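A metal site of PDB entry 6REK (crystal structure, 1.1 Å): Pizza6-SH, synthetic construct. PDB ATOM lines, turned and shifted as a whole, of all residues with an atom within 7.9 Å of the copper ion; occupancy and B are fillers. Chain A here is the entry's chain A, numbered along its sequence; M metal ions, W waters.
NE2 of His 203 lies close to OG1 of Thr 228 (3.2 Å).
O of Thr 186 sits at hydrogen-bond distance from N of His 203, at 3.1 Å.
The backbone NH (N) of His 245 is in hydrogen-bond range of the backbone carbonyl oxygen (O) of Thr 228 (2.9 Å).
N of His 230 sits at hydrogen-bond distance from O of Thr 243 (2.9 Å).
Of the 14 residues printed, 4 come within 4 Å of the copper ion.
The copper ion is bound by ND1 of His 245, at 2.0 Å.
NE2 of His 203 binds the copper ion (2.0 Å).
A ring nitrogen (NE2) of His 230 binds the copper ion, at 2.2 Å.
Water W1 binds the copper ion (2.3 Å).
Slightly farther from the copper ion lies the side-chain hydroxyl (OG1) of Thr 228 (2.7 Å).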
ATOM      1  N   THR A  18      -1.407   1.735 -19.861  1.00  0.00           N
ATOM      2  CA  THR A  18      -1.078   3.169 -19.944  1.00  0.00           C
ATOM      3  C   THR A  18      -1.906   3.855 -21.035  1.00  0.00           C
ATOM      4  O   THR A  18      -1.380   4.372 -22.017  1.00  0.00           O
ATOM      5  CB  THR A  18       0.426   3.438 -20.099  1.00  0.00           C
ATOM      6  OG1 THR A  18       1.106   2.649 -19.113  1.00  0.00           O
ATOM      7  CG2 THR A  18       0.790   4.905 -19.855  1.00  0.00           C
ATOM      8  N   PRO A  19      -3.222   3.948 -20.861  1.00  0.00           N
ATOM      9  CA  PRO A  19      -4.034   4.731 -21.812  1.00  0.00           C
ATOM     10  C   PRO A  19      -3.648   6.182 -21.655  1.00  0.00           C
ATOM     11  O   PRO A  19      -3.667   6.732 -20.550  1.00  0.00           O
ATOM     12  CB  PRO A  19      -5.481   4.475 -21.366  1.00  0.00           C
ATOM     13  CG  PRO A  19      -5.344   4.157 -19.886  1.00  0.00           C
ATOM     14  CD  PRO A  19      -4.027   3.388 -19.757  1.00  0.00           C
ATOM     15  N   THR A 186       1.792  19.107 -12.680  1.00  0.00           N
ATOM     16  CA  THR A 186       1.852  18.275 -13.888  1.00  0.00           C
ATOM     17  C   THR A 186       0.497  18.254 -14.601  1.00  0.00           C
ATOM     18  O   THR A 186      -0.116  17.186 -14.769  1.00  0.00           O
ATOM     19  CB  THR A 186       2.360  16.848 -13.601  1.00  0.00           C
ATOM     20  OG1 THR A 186       3.529  16.957 -12.784  1.00  0.00           O
ATOM     21  CG2 THR A 186       2.712  16.115 -14.876  1.00  0.00           C
ATOM     22  N   SER A 188      -1.660  17.649 -17.536  1.00  0.00           N
ATOM     23  CA  SER A 188      -1.414  16.785 -18.662  1.00  0.00           C
ATOM     24  C   SER A 188      -2.383  17.127 -19.789  1.00  0.00           C
ATOM     25  O   SER A 188      -2.089  17.835 -20.751  1.00  0.00           O
ATOM     26  CB  SER A 188      -1.496  15.336 -18.166  1.00  0.00           C
ATOM     27  OG  SER A 188      -1.013  14.487 -19.140  1.00  0.00           O
ATOM     28  N   HIS A 203      -2.280  15.727 -13.073  1.00  0.00           N
ATOM     29  CA  HIS A 203      -1.783  14.376 -12.932  1.00  0.00           C
ATOM     30  C   HIS A 203      -1.137  14.171 -11.565  1.00  0.00           C
ATOM     31  O   HIS A 203      -1.395  13.171 -10.878  1.00  0.00           O
ATOM     32  CB  HIS A 203      -0.781  14.088 -14.068  1.00  0.00           C
ATOM     33  CG  HIS A 203      -0.136  12.733 -14.008  1.00  0.00           C
ATOM     34  ND1 HIS A 203       1.000  12.467 -13.280  1.00  0.00           N
ATOM     35  CD2 HIS A 203      -0.421  11.586 -14.681  1.00  0.00           C
ATOM     36  CE1 HIS A 203       1.337  11.198 -13.439  1.00  0.00           C
ATOM     37  NE2 HIS A 203       0.492  10.635 -14.292  1.00  0.00           N
ATOM     38  N   GLY A 204      -0.312  15.130 -11.135  1.00  0.00           N
ATOM     39  CA  GLY A 204       0.401  15.010  -9.875  1.00  0.00           C
ATOM     40  C   GLY A 204      -0.472  15.195  -8.654  1.00  0.00           C
ATOM     41  O   GLY A 204      -0.037  14.874  -7.532  1.00  0.00           O
ATOM     42  N   ASN A 227      -6.209   6.697 -10.355  1.00  0.00           N
ATOM     43  CA  ASN A 227      -4.755   6.519 -10.047  1.00  0.00           C
ATOM     44  C   ASN A 227      -3.901   7.160 -11.157  1.00  0.00           C
ATOM     45  O   ASN A 227      -3.126   6.524 -11.880  1.00  0.00           O
ATOM     46  CB  ASN A 227      -4.362   5.080  -9.896  1.00  0.00           C
ATOM     47  CG  ASN A 227      -2.918   4.937  -9.421  1.00  0.00           C
ATOM     48  OD1 ASN A 227      -2.257   5.939  -9.195  1.00  0.00           O
ATOM     49  ND2 ASN A 227      -2.445   3.700  -9.241  1.00  0.00           N
ATOM     50  N   THR A 228      -4.018   8.439 -11.245  1.00  0.00           N
ATOM     51  CA  THR A 228      -3.367   9.475 -12.068  1.00  0.00           C
ATOM     52  C   THR A 228      -3.997   9.642 -13.458  1.00  0.00           C
ATOM     53  O   THR A 228      -3.854   8.793 -14.324  1.00  0.00           O
ATOM     54  CB  THR A 228      -1.832   9.442 -12.180  1.00  0.00           C
ATOM     55  OG1 THR A 228      -1.407   8.360 -12.981  1.00  0.00           O
ATOM     56  CG2 THR A 228      -1.158   9.430 -10.799  1.00  0.00           C
ATOM     57  N   PRO A 229      -4.730  10.697 -13.675  1.00  0.00           N
ATOM     58  CA  PRO A 229      -5.389  10.904 -14.963  1.00  0.00           C
ATOM     59  C   PRO A 229      -4.439  11.469 -16.007  1.00  0.00           C
ATOM     60  O   PRO A 229      -3.595  12.325 -15.692  1.00  0.00           O
ATOM     61  CB  PRO A 229      -6.466  11.939 -14.591  1.00  0.00           C
ATOM     62  CG  PRO A 229      -5.824  12.740 -13.466  1.00  0.00           C
ATOM     63  CD  PRO A 229      -5.008  11.749 -12.676  1.00  0.00           C
ATOM     64  N   HIS A 230      -4.603  11.018 -17.245  1.00  0.00           N
ATOM     65  CA  HIS A 230      -3.824  11.540 -18.367  1.00  0.00           C
ATOM     66  C   HIS A 230      -4.704  12.326 -19.338  1.00  0.00           C
ATOM     67  O   HIS A 230      -4.731  13.552 -19.354  1.00  0.00           O
ATOM     68  CB  HIS A 230      -3.063  10.440 -19.099  1.00  0.00           C
ATOM     69  CG  HIS A 230      -1.851   9.961 -18.356  1.00  0.00           C
ATOM     70  ND1 HIS A 230      -0.590   9.948 -18.897  1.00  0.00           N
ATOM     71  CD2 HIS A 230      -1.715   9.534 -17.074  1.00  0.00           C
ATOM     72  CE1 HIS A 230       0.266   9.478 -18.001  1.00  0.00           C
ATOM     73  NE2 HIS A 230      -0.392   9.227 -16.885  1.00  0.00           N
ATOM     74  N   THR A 243      -8.768   9.296 -19.162  1.00  0.00           N
ATOM     75  CA  THR A 243      -7.975   8.088 -19.065  1.00  0.00           C
ATOM     76  C   THR A 243      -7.280   8.045 -17.717  1.00  0.00           C
ATOM     77  O   THR A 243      -6.728   9.034 -17.227  1.00  0.00           O
ATOM     78  CB  THR A 243      -6.964   7.972 -20.216  1.00  0.00           C
ATOM     79  OG1 THR A 243      -5.900   8.929 -20.092  1.00  0.00           O
ATOM     80  CG2 THR A 243      -7.571   8.076 -21.573  1.00  0.00           C
ATOM     81  N   ASP A 244      -7.306   6.868 -17.093  1.00  0.00           N
ATOM     82  CA  ASP A 244      -6.829   6.641 -15.734  1.00  0.00           C
ATOM     83  C   ASP A 244      -5.610   5.723 -15.820  1.00  0.00           C
ATOM     84  O   ASP A 244      -5.758   4.503 -15.992  1.00  0.00           O
ATOM     85  CB  ASP A 244      -7.979   6.045 -14.897  1.00  0.00           C
ATOM     86  CG  ASP A 244      -7.638   5.787 -13.450  1.00  0.00           C
ATOM     87  OD1 ASP A 244      -6.498   6.021 -13.097  1.00  0.00           O
ATOM     88  OD2 ASP A 244      -8.545   5.277 -12.715  1.00  0.00           O
ATOM     89  N   HIS A 245      -4.418   6.309 -15.761  1.00  0.00           N
ATOM     90  CA  HIS A 245      -3.176   5.602 -16.021  1.00  0.00           C
ATOM     91  C   HIS A 245      -2.972   4.382 -15.154  1.00  0.00           C
ATOM     92  O   HIS A 245      -2.784   3.259 -15.654  1.00  0.00           O
ATOM     93  CB  HIS A 245      -2.036   6.622 -15.906  1.00  0.00           C
ATOM     94  CG  HIS A 245      -0.647   6.063 -15.872  1.00  0.00           C
ATOM     95  ND1 HIS A 245       0.404   6.825 -15.432  1.00  0.00           N
ATOM     96  CD2 HIS A 245      -0.138   4.863 -16.224  1.00  0.00           C
ATOM     97  CE1 HIS A 245       1.514   6.129 -15.517  1.00  0.00           C
ATOM     98  NE2 HIS A 245       1.212   4.931 -15.969  1.00  0.00           N
ATOM     99  N   GLY A 246      -2.950   4.554 -13.850  1.00  0.00           N
ATOM    100  CA  GLY A 246      -2.649   3.416 -12.963  1.00  0.00           C
ATOM    101  C   GLY A 246      -3.705   2.306 -12.899  1.00  0.00           C
ATOM    102  O   GLY A 246      -3.422   1.218 -12.390  1.00  0.00           O
HETATM  103 CU    CU M   1       0.421   8.714 -14.873  1.00  0.00          CU
HETATM  104  O   HOH W   1       1.663   8.117 -13.055  1.00  0.00           O
